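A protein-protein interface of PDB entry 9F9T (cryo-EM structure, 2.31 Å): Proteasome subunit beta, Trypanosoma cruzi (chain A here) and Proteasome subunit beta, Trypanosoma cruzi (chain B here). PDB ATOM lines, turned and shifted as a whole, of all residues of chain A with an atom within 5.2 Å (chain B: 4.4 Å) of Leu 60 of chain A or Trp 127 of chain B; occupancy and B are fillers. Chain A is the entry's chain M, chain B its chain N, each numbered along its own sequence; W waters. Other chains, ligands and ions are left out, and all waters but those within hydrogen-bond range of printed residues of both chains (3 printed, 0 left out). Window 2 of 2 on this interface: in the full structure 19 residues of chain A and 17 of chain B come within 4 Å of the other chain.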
ATOM      1  N   ASN A  39      35.857  28.983  23.696  1.00  0.00           N
ATOM      2  CA  ASN A  39      34.760  28.279  24.302  1.00  0.00           C
ATOM      3  C   ASN A  39      34.538  26.887  23.697  1.00  0.00           C
ATOM      4  O   ASN A  39      33.601  26.174  24.066  1.00  0.00           O
ATOM      5  CB  ASN A  39      33.552  29.193  24.276  1.00  0.00           C
ATOM      6  CG  ASN A  39      33.806  30.446  25.097  1.00  0.00           C
ATOM      7  OD1 ASN A  39      33.886  31.579  24.612  1.00  0.00           O
ATOM      8  ND2 ASN A  39      33.880  30.245  26.392  1.00  0.00           N
ATOM      9  N   THR A  58      26.394  22.060  20.711  1.00  0.00           N
ATOM     10  CA  THR A  58      25.731  22.964  21.646  1.00  0.00           C
ATOM     11  C   THR A  58      26.401  23.075  23.032  1.00  0.00           C
ATOM     12  O   THR A  58      25.922  23.778  23.881  1.00  0.00           O
ATOM     13  CB  THR A  58      24.277  22.548  21.912  1.00  0.00           C
ATOM     14  OG1 THR A  58      24.402  21.326  22.646  1.00  0.00           O
ATOM     15  CG2 THR A  58      23.498  22.442  20.633  1.00  0.00           C
ATOM     16  N   ARG A  59      27.608  22.633  23.162  1.00  0.00           N
ATOM     17  CA  ARG A  59      28.273  22.832  24.420  1.00  0.00           C
ATOM     18  C   ARG A  59      28.939  24.193  24.450  1.00  0.00           C
ATOM     19  O   ARG A  59      29.588  24.569  23.506  1.00  0.00           O
ATOM     20  CB  ARG A  59      29.287  21.686  24.579  1.00  0.00           C
ATOM     21  CG  ARG A  59      29.944  21.599  25.948  1.00  0.00           C
ATOM     22  CD  ARG A  59      30.850  20.402  26.040  1.00  0.00           C
ATOM     23  NE  ARG A  59      29.987  19.320  26.406  1.00  0.00           N
ATOM     24  CZ  ARG A  59      30.422  18.119  26.742  1.00  0.00           C
ATOM     25  NH1 ARG A  59      29.543  17.197  27.106  1.00  0.00           N
ATOM     26  NH2 ARG A  59      31.720  17.857  26.664  1.00  0.00           N
ATOM     27  N   LEU A  60      28.876  24.889  25.575  1.00  0.00           N
ATOM     28  CA  LEU A  60      29.702  26.066  25.761  1.00  0.00           C
ATOM     29  C   LEU A  60      30.624  25.848  26.922  1.00  0.00           C
ATOM     30  O   LEU A  60      30.157  25.711  28.015  1.00  0.00           O
ATOM     31  CB  LEU A  60      28.809  27.245  26.110  1.00  0.00           C
ATOM     32  CG  LEU A  60      29.455  28.646  26.107  1.00  0.00           C
ATOM     33  CD1 LEU A  60      29.836  29.082  24.707  1.00  0.00           C
ATOM     34  CD2 LEU A  60      28.475  29.659  26.686  1.00  0.00           C
ATOM     35  N   ASN A  61      31.902  25.844  26.640  1.00  0.00           N
ATOM     36  CA  ASN A  61      32.891  25.455  27.599  1.00  0.00           C
ATOM     37  C   ASN A  61      33.478  26.710  28.236  1.00  0.00           C
ATOM     38  O   ASN A  61      33.738  27.681  27.542  1.00  0.00           O
ATOM     39  CB  ASN A  61      34.068  24.653  26.986  1.00  0.00           C
ATOM     40  CG  ASN A  61      33.600  23.358  26.350  1.00  0.00           C
ATOM     41  OD1 ASN A  61      33.124  22.470  27.040  1.00  0.00           O
ATOM     42  ND2 ASN A  61      33.649  23.245  25.035  1.00  0.00           N
ATOM     43  N   GLY A  62      33.801  26.579  29.532  1.00  0.00           N
ATOM     44  CA  GLY A  62      34.673  27.508  30.247  1.00  0.00           C
ATOM     45  C   GLY A  62      36.062  26.925  30.484  1.00  0.00           C
ATOM     46  O   GLY A  62      36.478  26.025  29.749  1.00  0.00           O
ATOM     47  N   CYS A  65      35.485  23.507  32.834  1.00  0.00           N
ATOM     48  CA  CYS A  65      34.116  23.453  33.279  1.00  0.00           C
ATOM     49  C   CYS A  65      33.239  23.615  32.069  1.00  0.00           C
ATOM     50  O   CYS A  65      33.750  23.789  30.981  1.00  0.00           O
ATOM     51  CB  CYS A  65      33.780  24.485  34.361  1.00  0.00           C
ATOM     52  SG  CYS A  65      33.764  26.224  33.825  1.00  0.00           S
ATOM     53  N   ILE A  66      31.934  23.563  32.287  1.00  0.00           N
ATOM     54  CA  ILE A  66      30.976  23.724  31.233  1.00  0.00           C
ATOM     55  C   ILE A  66      29.921  24.725  31.661  1.00  0.00           C
ATOM     56  O   ILE A  66      29.172  24.471  32.595  1.00  0.00           O
ATOM     57  CB  ILE A  66      30.295  22.371  31.015  1.00  0.00           C
ATOM     58  CG1 ILE A  66      31.080  21.437  30.153  1.00  0.00           C
ATOM     59  CG2 ILE A  66      28.926  22.496  30.396  1.00  0.00           C
ATOM     60  CD1 ILE A  66      30.502  20.092  30.290  1.00  0.00           C
ATOM     61  N   HIS A  67      29.779  25.779  30.920  1.00  0.00           N
ATOM     62  CA  HIS A  67      28.796  26.744  31.255  1.00  0.00           C
ATOM     63  C   HIS A  67      27.468  26.135  30.948  1.00  0.00           C
ATOM     64  O   HIS A  67      26.580  26.127  31.799  1.00  0.00           O
ATOM     65  CB  HIS A  67      28.992  28.025  30.451  1.00  0.00           C
ATOM     66  CG  HIS A  67      30.244  28.727  30.832  1.00  0.00           C
ATOM     67  ND1 HIS A  67      30.635  28.818  32.150  1.00  0.00           N
ATOM     68  CD2 HIS A  67      31.181  29.378  30.087  1.00  0.00           C
ATOM     69  CE1 HIS A  67      31.807  29.460  32.182  1.00  0.00           C
ATOM     70  NE2 HIS A  67      32.168  29.788  30.948  1.00  0.00           N
ATOM     71  N   THR A  68      27.310  25.641  29.722  1.00  0.00           N
ATOM     72  CA  THR A  68      26.020  25.027  29.412  1.00  0.00           C
ATOM     73  C   THR A  68      26.117  24.027  28.290  1.00  0.00           C
ATOM     74  O   THR A  68      26.975  24.139  27.465  1.00  0.00           O
ATOM     75  CB  THR A  68      24.955  26.048  29.081  1.00  0.00           C
ATOM     76  OG1 THR A  68      23.798  25.321  28.729  1.00  0.00           O
ATOM     77  CG2 THR A  68      25.280  26.871  27.875  1.00  0.00           C
ATOM     78  N   ARG A  69      25.140  23.138  28.269  1.00  0.00           N
ATOM     79  CA  ARG A  69      24.996  22.138  27.236  1.00  0.00           C
ATOM     80  C   ARG A  69      23.965  22.509  26.164  1.00  0.00           C
ATOM     81  O   ARG A  69      23.701  21.683  25.301  1.00  0.00           O
ATOM     82  CB  ARG A  69      24.584  20.815  27.882  1.00  0.00           C
ATOM     83  CG  ARG A  69      25.659  20.176  28.742  1.00  0.00           C
ATOM     84  CD  ARG A  69      25.133  18.824  29.171  1.00  0.00           C
ATOM     85  NE  ARG A  69      25.474  18.492  30.547  1.00  0.00           N
ATOM     86  CZ  ARG A  69      26.603  17.959  30.972  1.00  0.00           C
ATOM     87  NH1 ARG A  69      26.883  18.020  32.261  1.00  0.00           N
ATOM     88  NH2 ARG A  69      27.464  17.440  30.130  1.00  0.00           N
ATOM     89  N   ASP A  71      23.865  25.918  24.251  1.00  0.00           N
ATOM     90  CA  ASP A  71      24.114  27.140  23.511  1.00  0.00           C
ATOM     91  C   ASP A  71      23.825  26.919  22.022  1.00  0.00           C
ATOM     92  O   ASP A  71      24.310  25.951  21.435  1.00  0.00           O
ATOM     93  CB  ASP A  71      25.576  27.572  23.676  1.00  0.00           C
ATOM     94  CG  ASP A  71      26.030  28.722  22.752  1.00  0.00           C
ATOM     95  OD1 ASP A  71      25.384  29.784  22.728  1.00  0.00           O
ATOM     96  OD2 ASP A  71      27.055  28.563  22.046  1.00  0.00           O
ATOM     97  N   GLN A  90      33.100  32.856  22.046  1.00  0.00           N
ATOM     98  CA  GLN A  90      31.715  33.077  21.801  1.00  0.00           C
ATOM     99  C   GLN A  90      31.382  34.556  21.840  1.00  0.00           C
ATOM    100  O   GLN A  90      30.477  34.998  21.173  1.00  0.00           O
ATOM    101  CB  GLN A  90      31.013  32.334  22.907  1.00  0.00           C
ATOM    102  CG  GLN A  90      29.532  32.336  22.670  1.00  0.00           C
ATOM    103  CD  GLN A  90      28.757  32.874  23.827  1.00  0.00           C
ATOM    104  OE1 GLN A  90      29.206  33.740  24.556  1.00  0.00           O
ATOM    105  NE2 GLN A  90      27.520  32.463  23.939  1.00  0.00           N
ATOM    106  N   ARG A  93      32.045  35.834  18.281  1.00  0.00           N
ATOM    107  CA  ARG A  93      31.020  35.459  17.324  1.00  0.00           C
ATOM    108  C   ARG A  93      29.744  36.228  17.558  1.00  0.00           C
ATOM    109  O   ARG A  93      29.175  36.585  16.586  1.00  0.00           O
ATOM    110  CB  ARG A  93      30.806  33.951  17.194  1.00  0.00           C
ATOM    111  CG  ARG A  93      29.835  33.315  18.166  1.00  0.00           C
ATOM    112  CD  ARG A  93      29.845  31.796  17.975  1.00  0.00           C
ATOM    113  NE  ARG A  93      29.499  31.049  19.145  1.00  0.00           N
ATOM    114  CZ  ARG A  93      30.355  30.226  19.710  1.00  0.00           C
ATOM    115  NH1 ARG A  93      29.965  29.424  20.681  1.00  0.00           N
ATOM    116  NH2 ARG A  93      31.607  30.155  19.336  1.00  0.00           N
ATOM    117  N   ASP A 224      27.147  16.912  23.619  1.00  0.00           N
ATOM    118  CA  ASP A 224      25.787  17.269  24.063  1.00  0.00           C
ATOM    119  C   ASP A 224      24.720  17.125  22.978  1.00  0.00           C
ATOM    120  O   ASP A 224      23.907  16.214  23.022  1.00  0.00           O
ATOM    121  CB  ASP A 224      25.697  18.654  24.668  1.00  0.00           C
ATOM    122  CG  ASP A 224      26.681  18.883  25.812  1.00  0.00           C
ATOM    123  OD1 ASP A 224      26.798  17.981  26.743  1.00  0.00           O
ATOM    124  OD2 ASP A 224      27.327  19.990  25.785  1.00  0.00           O
ATOM    125  N   PHE B  84      19.763  42.098  30.745  1.00  0.00           N
ATOM    126  CA  PHE B  84      20.839  41.166  30.511  1.00  0.00           C
ATOM    127  C   PHE B  84      21.602  41.472  29.236  1.00  0.00           C
ATOM    128  O   PHE B  84      22.796  41.521  29.181  1.00  0.00           O
ATOM    129  CB  PHE B  84      20.237  39.793  30.479  1.00  0.00           C
ATOM    130  CG  PHE B  84      21.239  38.677  30.355  1.00  0.00           C
ATOM    131  CD1 PHE B  84      21.983  38.323  31.464  1.00  0.00           C
ATOM    132  CD2 PHE B  84      21.363  37.950  29.161  1.00  0.00           C
ATOM    133  CE1 PHE B  84      22.878  37.297  31.422  1.00  0.00           C
ATOM    134  CE2 PHE B  84      22.276  36.930  29.106  1.00  0.00           C
ATOM    135  CZ  PHE B  84      22.996  36.568  30.241  1.00  0.00           C
ATOM    136  N   ARG B 104      32.190  38.511  37.244  1.00  0.00           N
ATOM    137  CA  ARG B 104      31.419  37.519  36.556  1.00  0.00           C
ATOM    138  C   ARG B 104      30.002  37.612  37.085  1.00  0.00           C
ATOM    139  O   ARG B 104      29.815  37.495  38.259  1.00  0.00           O
ATOM    140  CB  ARG B 104      32.142  36.186  36.774  1.00  0.00           C
ATOM    141  CG  ARG B 104      31.329  35.055  36.179  1.00  0.00           C
ATOM    142  CD  ARG B 104      32.110  33.885  35.597  1.00  0.00           C
ATOM    143  NE  ARG B 104      31.188  32.752  35.539  1.00  0.00           N
ATOM    144  CZ  ARG B 104      31.580  31.502  35.399  1.00  0.00           C
ATOM    145  NH1 ARG B 104      30.745  30.519  35.734  1.00  0.00           N
ATOM    146  NH2 ARG B 104      32.830  31.283  34.994  1.00  0.00           N
ATOM    147  N   GLY B 118      20.827  33.881  33.879  1.00  0.00           N
ATOM    148  CA  GLY B 118      21.938  33.862  32.936  1.00  0.00           C
ATOM    149  C   GLY B 118      23.230  34.399  33.530  1.00  0.00           C
ATOM    150  O   GLY B 118      23.288  34.883  34.641  1.00  0.00           O
ATOM    151  N   GLY B 119      24.309  34.202  32.787  1.00  0.00           N
ATOM    152  CA  GLY B 119      25.613  34.559  33.281  1.00  0.00           C
ATOM    153  C   GLY B 119      26.337  35.329  32.235  1.00  0.00           C
ATOM    154  O   GLY B 119      25.990  35.222  31.075  1.00  0.00           O
ATOM    155  N   VAL B 120      27.220  36.201  32.697  1.00  0.00           N
ATOM    156  CA  VAL B 120      28.076  36.946  31.814  1.00  0.00           C
ATOM    157  C   VAL B 120      29.447  36.952  32.411  1.00  0.00           C
ATOM    158  O   VAL B 120      29.540  37.421  33.545  1.00  0.00           O
ATOM    159  CB  VAL B 120      27.653  38.372  31.685  1.00  0.00           C
ATOM    160  CG1 VAL B 120      28.554  39.079  30.706  1.00  0.00           C
ATOM    161  CG2 VAL B 120      26.193  38.512  31.284  1.00  0.00           C
ATOM    162  N   ASP B 121      30.472  36.502  31.649  1.00  0.00           N
ATOM    163  CA  ASP B 121      31.801  36.604  32.183  1.00  0.00           C
ATOM    164  C   ASP B 121      32.599  37.809  31.691  1.00  0.00           C
ATOM    165  O   ASP B 121      32.106  38.608  30.922  1.00  0.00           O
ATOM    166  CB  ASP B 121      32.552  35.336  31.965  1.00  0.00           C
ATOM    167  CG  ASP B 121      33.143  35.176  30.607  1.00  0.00           C
ATOM    168  OD1 ASP B 121      32.950  36.102  29.742  1.00  0.00           O
ATOM    169  OD2 ASP B 121      33.815  34.167  30.402  1.00  0.00           O
ATOM    170  N   THR B 125      31.333  36.585  27.385  1.00  0.00           N
ATOM    171  CA  THR B 125      30.592  35.331  27.247  1.00  0.00           C
ATOM    172  C   THR B 125      29.267  35.319  27.996  1.00  0.00           C
ATOM    173  O   THR B 125      29.273  35.633  29.180  1.00  0.00           O
ATOM    174  CB  THR B 125      31.382  34.160  27.810  1.00  0.00           C
ATOM    175  OG1 THR B 125      32.742  34.340  27.464  1.00  0.00           O
ATOM    176  CG2 THR B 125      30.908  32.799  27.343  1.00  0.00           C
ATOM    177  N   ARG B 126      28.159  34.972  27.331  1.00  0.00           N
ATOM    178  CA  ARG B 126      26.861  34.914  27.981  1.00  0.00           C
ATOM    179  C   ARG B 126      26.123  33.629  27.694  1.00  0.00           C
ATOM    180  O   ARG B 126      26.224  33.087  26.617  1.00  0.00           O
ATOM    181  CB  ARG B 126      25.866  36.032  27.645  1.00  0.00           C
ATOM    182  CG  ARG B 126      25.999  36.531  26.243  1.00  0.00           C
ATOM    183  CD  ARG B 126      24.702  37.029  25.640  1.00  0.00           C
ATOM    184  NE  ARG B 126      23.501  36.265  25.767  1.00  0.00           N
ATOM    185  CZ  ARG B 126      22.284  36.846  25.785  1.00  0.00           C
ATOM    186  NH1 ARG B 126      22.125  38.151  25.557  1.00  0.00           N
ATOM    187  NH2 ARG B 126      21.211  36.119  26.042  1.00  0.00           N
ATOM    188  N   TRP B 127      25.355  33.189  28.665  1.00  0.00           N
ATOM    189  CA  TRP B 127      24.559  31.998  28.536  1.00  0.00           C
ATOM    190  C   TRP B 127      23.424  32.030  29.553  1.00  0.00           C
ATOM    191  O   TRP B 127      23.491  32.657  30.585  1.00  0.00           O
ATOM    192  CB  TRP B 127      25.432  30.770  28.759  1.00  0.00           C
ATOM    193  CG  TRP B 127      26.001  30.661  30.144  1.00  0.00           C
ATOM    194  CD1 TRP B 127      25.446  29.957  31.150  1.00  0.00           C
ATOM    195  CD2 TRP B 127      27.146  31.334  30.714  1.00  0.00           C
ATOM    196  NE1 TRP B 127      26.150  30.142  32.282  1.00  0.00           N
ATOM    197  CE2 TRP B 127      27.175  30.980  32.067  1.00  0.00           C
ATOM    198  CE3 TRP B 127      28.112  32.204  30.205  1.00  0.00           C
ATOM    199  CZ2 TRP B 127      28.123  31.434  32.950  1.00  0.00           C
ATOM    200  CZ3 TRP B 127      29.045  32.688  31.080  1.00  0.00           C
ATOM    201  CH2 TRP B 127      29.006  32.356  32.454  1.00  0.00           C
ATOM    202  N   THR B 128      22.326  31.408  29.207  1.00  0.00           N
ATOM    203  CA  THR B 128      21.200  31.239  30.103  1.00  0.00           C
ATOM    204  C   THR B 128      21.111  29.756  30.435  1.00  0.00           C
ATOM    205  O   THR B 128      21.650  28.964  29.717  1.00  0.00           O
ATOM    206  CB  THR B 128      19.929  31.830  29.458  1.00  0.00           C
ATOM    207  OG1 THR B 128      19.611  31.180  28.256  1.00  0.00           O
ATOM    208  CG2 THR B 128      20.173  33.259  29.102  1.00  0.00           C
ATOM    209  N   VAL B 132      23.082  28.431  37.126  1.00  0.00           N
ATOM    210  CA  VAL B 132      24.246  29.222  36.765  1.00  0.00           C
ATOM    211  C   VAL B 132      25.005  29.488  38.056  1.00  0.00           C
ATOM    212  O   VAL B 132      24.451  29.463  39.148  1.00  0.00           O
ATOM    213  CB  VAL B 132      23.750  30.546  36.113  1.00  0.00           C
ATOM    214  CG1 VAL B 132      24.842  31.545  35.688  1.00  0.00           C
ATOM    215  CG2 VAL B 132      22.864  30.283  34.885  1.00  0.00           C
HETATM  216  O   HOH W   1      33.853  28.840  35.417  1.00  0.00           O
HETATM  217  O   HOH W   2      30.091  27.899  34.482  1.00  0.00           O
HETATM  218  O   HOH W   3      33.459  34.193  25.158  1.00  0.00           O
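The side-chain amide nitrogen (NE2) of Gln 90 of chain A lies within hydrogen-bond range of the backbone carbonyl oxygen (O) of Arg 126 of chain B.
Of the 11 printed residues of chain B, 4 touch a printed residue of chain A. Printed residues of chain B that touch a printed residue of chain A: Arg 104, Thr 125, Arg 126 and Trp 127. Hydrophobic or aromatic side chains of chain A within 4 Å of the printed part of chain B: Leu 60 and His 67. Among the printed residues, 5 pairs touch across the chains.
Water W3 lies within hydrogen-bond range of OG1 of Thr 125 of chain B, OD1 of Asn 39 of chain A and N of Gln 90 of chain A. Water W2 lies within hydrogen-bond range of ND1 of His 67 of chain A and NH1 of Arg 104 of chain B. Water W1 lies within hydrogen-bond range of NH2 of Arg 104 of chain B (2.7 Å) and SG of Cys 65 of chain A (3.1 Å).
Of chain B, only Trp 127 (3.8 Å) comes within 4 Å of Leu 60 of chain A. Ile 66 of chain A touches none of the printed residues of chain B. Of the printed residues of chain B, His 67 of chain A touches Arg 104 (3.5 Å) and Trp 127 (3.7 Å). Of the printed residues of chain B, Gln 90 of chain A touches Thr 125 and Arg 126. Of the printed residues of chain A, Arg 104 of chain B touches His 67 (3.5 Å). Of the printed residues of chain A, Thr 125 of chain B touches Gln 90. Printed residues of chain A within 4 Å of Arg 126 of chain B: Gln 90. The nearest residue of chain B that does not touch Leu 60 of chain A is Thr 125 of chain B (4.03 Å).
N of Gln 90 of chain A lies within hydrogen-bond range of OD1 of Asn 39 of chain A (3.0 Å). The backbone carbonyl oxygen (O) of Leu 60 of chain A lies within hydrogen-bond range of the backbone NH (N) of His 67 of chain A, at 2.9 Å. The backbone NH of Leu 60 of chain A is in hydrogen-bond range of the backbone carbonyl oxygen of Thr 68 of chain A (2.8 Å). O of Trp 127 of chain B lies within hydrogen-bond range of N of Gly 119 of chain B, 2.8 Å away. The side-chain carboxylate (OD1) of Asp 121 of chain B sits at hydrogen-bond distance from the side-chain hydroxyl (OG1) of Thr 125 of chain B (2.9 Å).
Among the printed residues, pairs that only touch across the chains: Gln 90 of chain A with Thr 125 of chain B, His 67 of chain A with Arg 104 of chain B, His 67 of chain A with Trp 127 of chain B and Leu 60 of chain A with Trp 127 of chain B.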
